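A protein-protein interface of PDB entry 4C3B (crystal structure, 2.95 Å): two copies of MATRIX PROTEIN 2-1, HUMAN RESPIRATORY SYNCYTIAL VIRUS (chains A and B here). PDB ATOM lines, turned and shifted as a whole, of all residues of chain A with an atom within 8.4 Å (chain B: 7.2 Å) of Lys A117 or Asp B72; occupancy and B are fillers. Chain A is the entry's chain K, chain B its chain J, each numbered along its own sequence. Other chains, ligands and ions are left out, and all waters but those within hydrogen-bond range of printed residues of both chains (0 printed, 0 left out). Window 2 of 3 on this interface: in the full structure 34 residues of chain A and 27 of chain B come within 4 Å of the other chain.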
ATOM      1  N   ASN A 112      -8.865  14.794  25.874  1.00  0.00           N
ATOM      2  CA  ASN A 112      -8.176  13.781  26.645  1.00  0.00           C
ATOM      3  C   ASN A 112      -8.630  12.326  26.392  1.00  0.00           C
ATOM      4  O   ASN A 112      -9.813  11.973  26.489  1.00  0.00           O
ATOM      5  CB  ASN A 112      -8.168  14.165  28.130  1.00  0.00           C
ATOM      6  CG  ASN A 112      -9.411  13.723  28.857  1.00  0.00           C
ATOM      7  OD1 ASN A 112     -10.530  14.011  28.440  1.00  0.00           O
ATOM      8  ND2 ASN A 112      -9.216  13.005  29.952  1.00  0.00           N
ATOM      9  N   SER A 113      -7.642  11.482  26.097  1.00  0.00           N
ATOM     10  CA  SER A 113      -7.875  10.081  25.784  1.00  0.00           C
ATOM     11  C   SER A 113      -8.921   9.459  26.661  1.00  0.00           C
ATOM     12  O   SER A 113      -9.795   8.777  26.162  1.00  0.00           O
ATOM     13  CB  SER A 113      -6.608   9.280  25.921  1.00  0.00           C
ATOM     14  OG  SER A 113      -5.640   9.777  25.032  1.00  0.00           O
ATOM     15  N   ASP A 114      -8.860   9.696  27.959  1.00  0.00           N
ATOM     16  CA  ASP A 114      -9.817   9.040  28.837  1.00  0.00           C
ATOM     17  C   ASP A 114     -11.268   9.282  28.474  1.00  0.00           C
ATOM     18  O   ASP A 114     -12.055   8.355  28.508  1.00  0.00           O
ATOM     19  CB  ASP A 114      -9.569   9.366  30.298  1.00  0.00           C
ATOM     20  CG  ASP A 114      -8.648   8.383  30.921  1.00  0.00           C
ATOM     21  OD1 ASP A 114      -7.418   8.482  30.709  1.00  0.00           O
ATOM     22  OD2 ASP A 114      -9.175   7.455  31.569  1.00  0.00           O
ATOM     23  N   ASP A 115     -11.624  10.497  28.091  1.00  0.00           N
ATOM     24  CA  ASP A 115     -12.994  10.760  27.686  1.00  0.00           C
ATOM     25  C   ASP A 115     -13.412   9.930  26.447  1.00  0.00           C
ATOM     26  O   ASP A 115     -14.561   9.464  26.371  1.00  0.00           O
ATOM     27  CB  ASP A 115     -13.195  12.253  27.449  1.00  0.00           C
ATOM     28  CG  ASP A 115     -13.371  13.013  28.727  1.00  0.00           C
ATOM     29  OD1 ASP A 115     -13.880  12.422  29.690  1.00  0.00           O
ATOM     30  OD2 ASP A 115     -13.084  14.220  28.753  1.00  0.00           O
ATOM     31  N   ILE A 116     -12.481   9.736  25.500  1.00  0.00           N
ATOM     32  CA  ILE A 116     -12.728   8.918  24.306  1.00  0.00           C
ATOM     33  C   ILE A 116     -12.904   7.453  24.728  1.00  0.00           C
ATOM     34  O   ILE A 116     -13.851   6.779  24.313  1.00  0.00           O
ATOM     35  CB  ILE A 116     -11.566   8.934  23.286  1.00  0.00           C
ATOM     36  CG1 ILE A 116     -11.026  10.328  23.004  1.00  0.00           C
ATOM     37  CG2 ILE A 116     -11.985   8.282  21.972  1.00  0.00           C
ATOM     38  CD1 ILE A 116     -11.913  11.192  22.168  1.00  0.00           C
ATOM     39  N   LYS A 117     -11.979   6.943  25.535  1.00  0.00           N
ATOM     40  CA  LYS A 117     -12.079   5.578  26.019  1.00  0.00           C
ATOM     41  C   LYS A 117     -13.446   5.322  26.657  1.00  0.00           C
ATOM     42  O   LYS A 117     -14.052   4.270  26.424  1.00  0.00           O
ATOM     43  CB  LYS A 117     -10.977   5.267  27.014  1.00  0.00           C
ATOM     44  CG  LYS A 117      -9.619   5.178  26.362  1.00  0.00           C
ATOM     45  CD  LYS A 117      -8.481   5.004  27.362  1.00  0.00           C
ATOM     46  CE  LYS A 117      -7.180   4.925  26.566  1.00  0.00           C
ATOM     47  NZ  LYS A 117      -5.971   5.016  27.394  1.00  0.00           N
ATOM     48  N   LYS A 118     -13.937   6.295  27.410  1.00  0.00           N
ATOM     49  CA  LYS A 118     -15.258   6.209  27.992  1.00  0.00           C
ATOM     50  C   LYS A 118     -16.344   6.051  26.914  1.00  0.00           C
ATOM     51  O   LYS A 118     -17.291   5.292  27.113  1.00  0.00           O
ATOM     52  CB  LYS A 118     -15.526   7.434  28.846  1.00  0.00           C
ATOM     53  CG  LYS A 118     -16.981   7.726  29.167  1.00  0.00           C
ATOM     54  CD  LYS A 118     -17.560   6.710  30.131  1.00  0.00           C
ATOM     55  CE  LYS A 118     -18.984   7.089  30.513  1.00  0.00           C
ATOM     56  NZ  LYS A 118     -19.660   5.961  31.209  1.00  0.00           N
ATOM     57  N   LEU A 119     -16.180   6.716  25.766  1.00  0.00           N
ATOM     58  CA  LEU A 119     -17.156   6.629  24.675  1.00  0.00           C
ATOM     59  C   LEU A 119     -17.041   5.293  23.950  1.00  0.00           C
ATOM     60  O   LEU A 119     -18.052   4.676  23.608  1.00  0.00           O
ATOM     61  CB  LEU A 119     -16.952   7.732  23.647  1.00  0.00           C
ATOM     62  CG  LEU A 119     -17.218   9.192  24.009  1.00  0.00           C
ATOM     63  CD1 LEU A 119     -16.779  10.014  22.814  1.00  0.00           C
ATOM     64  CD2 LEU A 119     -18.673   9.472  24.352  1.00  0.00           C
ATOM     65  N   ARG A 120     -15.806   4.861  23.704  1.00  0.00           N
ATOM     66  CA  ARG A 120     -15.538   3.567  23.104  1.00  0.00           C
ATOM     67  C   ARG A 120     -16.176   2.426  23.893  1.00  0.00           C
ATOM     68  O   ARG A 120     -16.567   1.410  23.342  1.00  0.00           O
ATOM     69  CB  ARG A 120     -14.036   3.367  23.041  1.00  0.00           C
ATOM     70  CG  ARG A 120     -13.565   2.144  22.272  1.00  0.00           C
ATOM     71  CD  ARG A 120     -12.050   2.053  22.333  1.00  0.00           C
ATOM     72  NE  ARG A 120     -11.634   1.831  23.714  1.00  0.00           N
ATOM     73  CZ  ARG A 120     -10.374   1.845  24.149  1.00  0.00           C
ATOM     74  NH1 ARG A 120      -9.362   2.067  23.313  1.00  0.00           N
ATOM     75  NH2 ARG A 120     -10.139   1.622  25.442  1.00  0.00           N
ATOM     76  N   ASP A 121     -16.253   2.581  25.199  1.00  0.00           N
ATOM     77  CA  ASP A 121     -16.858   1.554  26.012  1.00  0.00           C
ATOM     78  C   ASP A 121     -18.344   1.466  25.821  1.00  0.00           C
ATOM     79  O   ASP A 121     -18.919   0.429  26.095  1.00  0.00           O
ATOM     80  CB  ASP A 121     -16.548   1.773  27.478  1.00  0.00           C
ATOM     81  CG  ASP A 121     -15.905   0.561  28.098  1.00  0.00           C
ATOM     82  OD1 ASP A 121     -14.726   0.281  27.774  1.00  0.00           O
ATOM     83  OD2 ASP A 121     -16.591  -0.097  28.904  1.00  0.00           O
ATOM     84  N   ASN A 122     -18.984   2.540  25.376  1.00  0.00           N
ATOM     85  CA  ASN A 122     -20.425   2.488  25.121  1.00  0.00           C
ATOM     86  C   ASN A 122     -20.746   1.840  23.797  1.00  0.00           C
ATOM     87  O   ASN A 122     -21.910   1.540  23.532  1.00  0.00           O
ATOM     88  CB  ASN A 122     -21.051   3.883  25.127  1.00  0.00           C
ATOM     89  CG  ASN A 122     -21.072   4.504  26.497  1.00  0.00           C
ATOM     90  OD1 ASN A 122     -20.582   5.621  26.699  1.00  0.00           O
ATOM     91  ND2 ASN A 122     -21.647   3.782  27.457  1.00  0.00           N
ATOM     92  N   GLU A 123     -19.741   1.618  22.959  1.00  0.00           N
ATOM     93  CA  GLU A 123     -19.988   1.035  21.653  1.00  0.00           C
ATOM     94  C   GLU A 123     -20.004  -0.489  21.744  1.00  0.00           C
ATOM     95  O   GLU A 123     -19.264  -1.084  22.540  1.00  0.00           O
ATOM     96  CB  GLU A 123     -18.934   1.498  20.644  1.00  0.00           C
ATOM     97  CG  GLU A 123     -19.098   2.933  20.197  1.00  0.00           C
ATOM     98  CD  GLU A 123     -20.428   3.175  19.507  1.00  0.00           C
ATOM     99  OE1 GLU A 123     -20.765   2.438  18.563  1.00  0.00           O
ATOM    100  OE2 GLU A 123     -21.141   4.102  19.913  1.00  0.00           O
ATOM    101  N   ILE A 130     -15.692   2.418  16.870  1.00  0.00           N
ATOM    102  CA  ILE A 130     -14.551   1.964  17.626  1.00  0.00           C
ATOM    103  C   ILE A 130     -13.232   2.106  16.850  1.00  0.00           C
ATOM    104  O   ILE A 130     -12.228   2.461  17.439  1.00  0.00           O
ATOM    105  CB  ILE A 130     -14.778   0.529  18.114  1.00  0.00           C
ATOM    106  CG1 ILE A 130     -15.885   0.559  19.172  1.00  0.00           C
ATOM    107  CG2 ILE A 130     -13.498  -0.074  18.667  1.00  0.00           C
ATOM    108  CD1 ILE A 130     -16.402  -0.795  19.621  1.00  0.00           C
ATOM    109  N   TYR A 133     -12.570   6.114  17.017  1.00  0.00           N
ATOM    110  CA  TYR A 133     -12.123   6.363  18.366  1.00  0.00           C
ATOM    111  C   TYR A 133     -10.680   5.960  18.591  1.00  0.00           C
ATOM    112  O   TYR A 133      -9.903   6.725  19.160  1.00  0.00           O
ATOM    113  CB  TYR A 133     -12.987   5.625  19.360  1.00  0.00           C
ATOM    114  CG  TYR A 133     -14.380   6.141  19.516  1.00  0.00           C
ATOM    115  CD1 TYR A 133     -14.704   7.442  19.243  1.00  0.00           C
ATOM    116  CD2 TYR A 133     -15.360   5.334  20.016  1.00  0.00           C
ATOM    117  CE1 TYR A 133     -15.984   7.917  19.471  1.00  0.00           C
ATOM    118  CE2 TYR A 133     -16.644   5.798  20.253  1.00  0.00           C
ATOM    119  CZ  TYR A 133     -16.956   7.091  19.976  1.00  0.00           C
ATOM    120  OH  TYR A 133     -18.242   7.538  20.196  1.00  0.00           O
ATOM    121  N   ASN A 134     -10.282   4.768  18.190  1.00  0.00           N
ATOM    122  CA  ASN A 134      -8.892   4.364  18.462  1.00  0.00           C
ATOM    123  C   ASN A 134      -7.926   5.162  17.616  1.00  0.00           C
ATOM    124  O   ASN A 134      -6.781   5.369  18.045  1.00  0.00           O
ATOM    125  CB  ASN A 134      -8.631   2.851  18.271  1.00  0.00           C
ATOM    126  CG  ASN A 134      -9.447   1.981  19.225  1.00  0.00           C
ATOM    127  OD1 ASN A 134      -9.545   2.236  20.450  1.00  0.00           O
ATOM    128  ND2 ASN A 134     -10.048   0.947  18.670  1.00  0.00           N
ATOM    129  N   ILE A 137      -7.578   8.478  19.400  1.00  0.00           N
ATOM    130  CA  ILE A 137      -6.826   8.237  20.625  1.00  0.00           C
ATOM    131  C   ILE A 137      -5.366   8.134  20.325  1.00  0.00           C
ATOM    132  O   ILE A 137      -4.566   8.707  21.027  1.00  0.00           O
ATOM    133  CB  ILE A 137      -7.298   6.986  21.348  1.00  0.00           C
ATOM    134  CG1 ILE A 137      -8.589   7.318  22.112  1.00  0.00           C
ATOM    135  CG2 ILE A 137      -6.232   6.511  22.308  1.00  0.00           C
ATOM    136  CD1 ILE A 137      -9.320   6.130  22.745  1.00  0.00           C
ATOM    137  N   SER A 138      -4.989   7.396  19.292  1.00  0.00           N
ATOM    138  CA  SER A 138      -3.559   7.237  19.010  1.00  0.00           C
ATOM    139  C   SER A 138      -2.977   8.557  18.573  1.00  0.00           C
ATOM    140  O   SER A 138      -1.843   8.861  18.910  1.00  0.00           O
ATOM    141  CB  SER A 138      -3.270   6.115  17.998  1.00  0.00           C
ATOM    142  OG  SER A 138      -4.209   6.134  16.946  1.00  0.00           O
ATOM    143  N   ILE A 140      -4.069  11.641  19.623  1.00  0.00           N
ATOM    144  CA  ILE A 140      -3.898  12.337  20.896  1.00  0.00           C
ATOM    145  C   ILE A 140      -2.575  11.967  21.588  1.00  0.00           C
ATOM    146  O   ILE A 140      -1.893  12.844  22.110  1.00  0.00           O
ATOM    147  CB  ILE A 140      -5.048  12.045  21.853  1.00  0.00           C
ATOM    148  CG1 ILE A 140      -6.320  12.723  21.337  1.00  0.00           C
ATOM    149  CG2 ILE A 140      -4.708  12.520  23.261  1.00  0.00           C
ATOM    150  CD1 ILE A 140      -7.573  12.490  22.167  1.00  0.00           C
ATOM    151  N   GLU A 141      -2.238  10.675  21.606  1.00  0.00           N
ATOM    152  CA  GLU A 141      -1.030  10.207  22.272  1.00  0.00           C
ATOM    153  C   GLU A 141       0.227  10.597  21.502  1.00  0.00           C
ATOM    154  O   GLU A 141       1.187  10.992  22.119  1.00  0.00           O
ATOM    155  CB  GLU A 141      -1.083   8.690  22.542  1.00  0.00           C
ATOM    156  CG  GLU A 141      -2.246   8.195  23.424  1.00  0.00           C
ATOM    157  CD  GLU A 141      -2.391   8.932  24.763  1.00  0.00           C
ATOM    158  OE1 GLU A 141      -1.448   9.621  25.200  1.00  0.00           O
ATOM    159  OE2 GLU A 141      -3.451   8.839  25.411  1.00  0.00           O
ATOM    160  N   ARG A 144       0.718  14.313  22.431  1.00  0.00           N
ATOM    161  CA  ARG A 144       1.293  14.568  23.749  1.00  0.00           C
ATOM    162  C   ARG A 144       2.794  14.243  23.771  1.00  0.00           C
ATOM    163  O   ARG A 144       3.563  14.981  24.368  1.00  0.00           O
ATOM    164  CB  ARG A 144       0.576  13.801  24.864  1.00  0.00           C
ATOM    165  CG  ARG A 144       0.695  14.489  26.226  1.00  0.00           C
ATOM    166  CD  ARG A 144       0.787  13.512  27.399  1.00  0.00           C
ATOM    167  NE  ARG A 144      -0.208  12.452  27.297  1.00  0.00           N
ATOM    168  CZ  ARG A 144      -1.505  12.595  27.564  1.00  0.00           C
ATOM    169  NH1 ARG A 144      -1.994  13.759  27.980  1.00  0.00           N
ATOM    170  NH2 ARG A 144      -2.328  11.558  27.409  1.00  0.00           N
ATOM    171  N   ILE A 172     -16.280  14.326  17.868  1.00  0.00           N
ATOM    172  CA  ILE A 172     -16.021  13.800  19.210  1.00  0.00           C
ATOM    173  C   ILE A 172     -15.918  14.934  20.209  1.00  0.00           C
ATOM    174  O   ILE A 172     -16.644  14.974  21.207  1.00  0.00           O
ATOM    175  CB  ILE A 172     -14.706  13.038  19.236  1.00  0.00           C
ATOM    176  CG1 ILE A 172     -14.891  11.682  18.562  1.00  0.00           C
ATOM    177  CG2 ILE A 172     -14.247  12.849  20.649  1.00  0.00           C
ATOM    178  CD1 ILE A 172     -13.589  11.080  18.101  1.00  0.00           C
ATOM    179  N   ILE A 176     -18.399  14.940  23.332  1.00  0.00           N
ATOM    180  CA  ILE A 176     -17.948  14.955  24.717  1.00  0.00           C
ATOM    181  C   ILE A 176     -18.508  16.157  25.471  1.00  0.00           C
ATOM    182  O   ILE A 176     -19.022  16.023  26.567  1.00  0.00           O
ATOM    183  CB  ILE A 176     -16.431  15.044  24.775  1.00  0.00           C
ATOM    184  CG1 ILE A 176     -15.813  13.738  24.337  1.00  0.00           C
ATOM    185  CG2 ILE A 176     -15.966  15.353  26.181  1.00  0.00           C
ATOM    186  CD1 ILE A 176     -14.309  13.808  24.110  1.00  0.00           C
ATOM    187  N   LYS B  53      -1.854  15.374  34.154  1.00  0.00           N
ATOM    188  CA  LYS B  53      -1.571  14.513  33.015  1.00  0.00           C
ATOM    189  C   LYS B  53      -0.341  15.018  32.300  1.00  0.00           C
ATOM    190  O   LYS B  53       0.492  14.261  31.816  1.00  0.00           O
ATOM    191  CB  LYS B  53      -2.750  14.439  32.038  1.00  0.00           C
ATOM    192  CG  LYS B  53      -3.462  13.089  32.048  1.00  0.00           C
ATOM    193  CD  LYS B  53      -4.392  12.849  30.847  1.00  0.00           C
ATOM    194  CE  LYS B  53      -5.045  11.453  30.884  1.00  0.00           C
ATOM    195  NZ  LYS B  53      -6.165  11.268  29.900  1.00  0.00           N
ATOM    196  N   ALA B  69       0.396  -0.894  27.199  1.00  0.00           N
ATOM    197  CA  ALA B  69      -0.537  -0.592  26.115  1.00  0.00           C
ATOM    198  C   ALA B  69      -1.679  -1.609  26.113  1.00  0.00           C
ATOM    199  O   ALA B  69      -2.798  -1.336  25.635  1.00  0.00           O
ATOM    200  CB  ALA B  69       0.187  -0.575  24.765  1.00  0.00           C
ATOM    201  N   GLU B  70      -1.358  -2.792  26.627  1.00  0.00           N
ATOM    202  CA  GLU B  70      -2.280  -3.919  26.777  1.00  0.00           C
ATOM    203  C   GLU B  70      -3.556  -3.577  27.545  1.00  0.00           C
ATOM    204  O   GLU B  70      -4.663  -3.901  27.093  1.00  0.00           O
ATOM    205  CB  GLU B  70      -1.544  -5.056  27.490  1.00  0.00           C
ATOM    206  CG  GLU B  70      -1.820  -6.448  26.950  1.00  0.00           C
ATOM    207  CD  GLU B  70      -0.619  -7.355  27.128  1.00  0.00           C
ATOM    208  OE1 GLU B  70       0.480  -6.931  26.714  1.00  0.00           O
ATOM    209  OE2 GLU B  70      -0.762  -8.468  27.693  1.00  0.00           O
ATOM    210  N   LEU B  71      -3.406  -2.924  28.698  1.00  0.00           N
ATOM    211  CA  LEU B  71      -4.559  -2.657  29.580  1.00  0.00           C
ATOM    212  C   LEU B  71      -5.382  -1.385  29.234  1.00  0.00           C
ATOM    213  O   LEU B  71      -6.220  -0.952  30.038  1.00  0.00           O
ATOM    214  CB  LEU B  71      -4.158  -2.741  31.080  1.00  0.00           C
ATOM    215  CG  LEU B  71      -3.158  -1.796  31.778  1.00  0.00           C
ATOM    216  CD1 LEU B  71      -3.879  -0.735  32.597  1.00  0.00           C
ATOM    217  CD2 LEU B  71      -2.217  -2.563  32.697  1.00  0.00           C
ATOM    218  N   ASP B  72      -5.141  -0.826  28.035  1.00  0.00           N
ATOM    219  CA  ASP B  72      -6.050   0.136  27.356  1.00  0.00           C
ATOM    220  C   ASP B  72      -7.215  -0.583  26.673  1.00  0.00           C
ATOM    221  O   ASP B  72      -8.277   0.014  26.449  1.00  0.00           O
ATOM    222  CB  ASP B  72      -5.313   0.950  26.281  1.00  0.00           C
ATOM    223  CG  ASP B  72      -4.412   2.016  26.857  1.00  0.00           C
ATOM    224  OD1 ASP B  72      -4.605   2.438  28.013  1.00  0.00           O
ATOM    225  OD2 ASP B  72      -3.481   2.438  26.147  1.00  0.00           O
ATOM    226  N   ARG B  73      -6.983  -1.855  26.329  1.00  0.00           N
ATOM    227  CA  ARG B  73      -7.966  -2.722  25.645  1.00  0.00           C
ATOM    228  C   ARG B  73      -9.314  -2.776  26.353  1.00  0.00           C
ATOM    229  O   ARG B  73      -9.382  -2.653  27.551  1.00  0.00           O
ATOM    230  CB  ARG B  73      -7.427  -4.146  25.507  1.00  0.00           C
ATOM    231  CG  ARG B  73      -6.717  -4.405  24.180  1.00  0.00           C
ATOM    232  CD  ARG B  73      -6.041  -5.768  24.127  1.00  0.00           C
ATOM    233  NE  ARG B  73      -6.501  -6.639  25.211  1.00  0.00           N
ATOM    234  CZ  ARG B  73      -5.742  -7.524  25.846  1.00  0.00           C
ATOM    235  NH1 ARG B  73      -4.465  -7.683  25.520  1.00  0.00           N
ATOM    236  NH2 ARG B  73      -6.267  -8.253  26.830  1.00  0.00           N
ATOM    237  N   THR B  74     -10.380  -2.978  25.590  1.00  0.00           N
ATOM    238  CA  THR B  74     -11.755  -2.757  26.077  1.00  0.00           C
ATOM    239  C   THR B  74     -12.106  -3.305  27.474  1.00  0.00           C
ATOM    240  O   THR B  74     -12.797  -2.607  28.232  1.00  0.00           O
ATOM    241  CB  THR B  74     -12.801  -3.236  25.036  1.00  0.00           C
ATOM    242  OG1 THR B  74     -12.758  -2.361  23.900  1.00  0.00           O
ATOM    243  CG2 THR B  74     -14.238  -3.240  25.603  1.00  0.00           C
ATOM    244  N   GLU B  75     -11.660  -4.510  27.834  1.00  0.00           N
ATOM    245  CA  GLU B  75     -12.104  -5.075  29.119  1.00  0.00           C
ATOM    246  C   GLU B  75     -11.162  -4.755  30.295  1.00  0.00           C
ATOM    247  O   GLU B  75     -11.593  -4.637  31.437  1.00  0.00           O
ATOM    248  CB  GLU B  75     -12.432  -6.559  28.993  1.00  0.00           C
ATOM    249  CG  GLU B  75     -11.351  -7.542  29.382  1.00  0.00           C
ATOM    250  CD  GLU B  75     -11.933  -8.933  29.556  1.00  0.00           C
ATOM    251  OE1 GLU B  75     -13.045  -9.181  29.038  1.00  0.00           O
ATOM    252  OE2 GLU B  75     -11.284  -9.783  30.206  1.00  0.00           O
ATOM    253  N   GLU B  76      -9.888  -4.539  29.997  1.00  0.00           N
ATOM    254  CA  GLU B  76      -8.926  -4.091  31.016  1.00  0.00           C
ATOM    255  C   GLU B  76      -9.219  -2.636  31.415  1.00  0.00           C
ATOM    256  O   GLU B  76      -8.852  -2.177  32.474  1.00  0.00           O
ATOM    257  CB  GLU B  76      -7.502  -4.281  30.485  1.00  0.00           C
ATOM    258  CG  GLU B  76      -7.375  -5.573  29.665  1.00  0.00           C
ATOM    259  CD  GLU B  76      -5.990  -6.194  29.661  1.00  0.00           C
ATOM    260  OE1 GLU B  76      -5.472  -6.568  30.739  1.00  0.00           O
ATOM    261  OE2 GLU B  76      -5.419  -6.338  28.561  1.00  0.00           O
ATOM    262  N   TYR B  77      -9.919  -1.919  30.552  1.00  0.00           N
ATOM    263  CA  TYR B  77     -10.425  -0.603  30.885  1.00  0.00           C
ATOM    264  C   TYR B  77     -11.623  -0.743  31.834  1.00  0.00           C
ATOM    265  O   TYR B  77     -11.718   0.012  32.781  1.00  0.00           O
ATOM    266  CB  TYR B  77     -10.789   0.220  29.618  1.00  0.00           C
ATOM    267  CG  TYR B  77     -11.646   1.460  29.883  1.00  0.00           C
ATOM    268  CD1 TYR B  77     -13.055   1.358  29.915  1.00  0.00           C
ATOM    269  CD2 TYR B  77     -11.071   2.716  30.103  1.00  0.00           C
ATOM    270  CE1 TYR B  77     -13.863   2.460  30.166  1.00  0.00           C
ATOM    271  CE2 TYR B  77     -11.876   3.830  30.355  1.00  0.00           C
ATOM    272  CZ  TYR B  77     -13.275   3.696  30.379  1.00  0.00           C
ATOM    273  OH  TYR B  77     -14.113   4.771  30.621  1.00  0.00           O
ATOM    274  N   ALA B  78     -12.542  -1.678  31.576  1.00  0.00           N
ATOM    275  CA  ALA B  78     -13.790  -1.784  32.377  1.00  0.00           C
ATOM    276  C   ALA B  78     -13.517  -2.386  33.738  1.00  0.00           C
ATOM    277  O   ALA B  78     -14.291  -2.209  34.687  1.00  0.00           O
ATOM    278  CB  ALA B  78     -14.844  -2.612  31.653  1.00  0.00           C
ATOM    279  N   LYS B 106       0.543   2.008  38.411  1.00  0.00           N
ATOM    280  CA  LYS B 106      -0.508   3.006  38.374  1.00  0.00           C
ATOM    281  C   LYS B 106      -1.137   3.156  39.768  1.00  0.00           C
ATOM    282  O   LYS B 106      -1.574   4.224  40.149  1.00  0.00           O
ATOM    283  CB  LYS B 106      -1.600   2.653  37.326  1.00  0.00           C
ATOM    284  CG  LYS B 106      -1.121   2.219  35.930  1.00  0.00           C
ATOM    285  CD  LYS B 106      -0.830   3.358  34.957  1.00  0.00           C
ATOM    286  CE  LYS B 106      -2.050   3.760  34.126  1.00  0.00           C
ATOM    287  NZ  LYS B 106      -2.465   2.684  33.181  1.00  0.00           N
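Among the printed residues, merely in contact across the chains: Asp A121 with Tyr B77, Lys A118 with Tyr B77, Asp A121 with Thr B74, Asn A112 with Lys B53, Lys A117 with Tyr B77 and Arg A144 with Lys B53.
The guanidinium group (NH2) of Arg A144 lies within salt-bridge range of the side-chain carboxylate (OE1) of Glu A141 (3.1 Å). OD1 of Asn A112 sits close to OD2 of Asp A115, at 2.6 Å. The backbone carbonyl oxygen (O) of Lys A118 sits close to the side-chain amide oxygen (OD1) of Asn A122 (3.3 Å). The side-chain amide oxygen (OD1) of Asn A134 lies within hydrogen-bond range of the guanidinium group (NH1) of Arg A120.
No position is printed for both chains. Of the 9 pairs that touch across the chains among the printed residues, none has its exchanged pair printed and touching as well.
The backbone carbonyl oxygen of Asp B72 is in hydrogen-bond range of the guanidinium group of Arg A120. OD1 of Asp B72 is in salt-bridge range of NZ of Lys A117 (3.0 Å). NZ of Lys B53 lies within salt-bridge range of OD1 of Asp A114 (3.2 Å).
Of the 12 printed residues of chain B, 4 touch a printed residue of chain A. Printed residues of chain B that touch a printed residue of chain A: Lys B53, Asp B72, Thr B74 and Tyr B77. Hydrophobic or aromatic side chains of chain B that line the printed part of chain A: Tyr B77. Along chain B the printed residues that touch a printed residue of chain A span positions 53 to 77. Among the printed residues, 9 pairs touch across the chains. Among the printed residues, Asp or Glu carboxylates within 4 Å of a Lys or Arg side-chain nitrogen of the other chain: Asp A114 with Lys B53 and Lys A117 with Asp B72.
Lys A117 touches just these residues of chain B: Asp B72 and Tyr B77. Of chain A, only Lys A117 and Arg A120 come within 4 Å of Asp B72. Of the printed residues of chain A, Tyr B77 touches Lys A117 (3.7 Å), Lys A118 (3.2 Å) and Asp A121 (2.9 Å). Printed residues of chain B within 4 Å of Asp A121: Thr B74 and Tyr B77. Of the printed residues of chain B, Asn A112 touches Lys B53. Of the printed residues of chain B, Asp A114 touches Lys B53. The nearest printed residue of chain A that does not touch Thr B74 is Arg A120 (4.3 Å).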
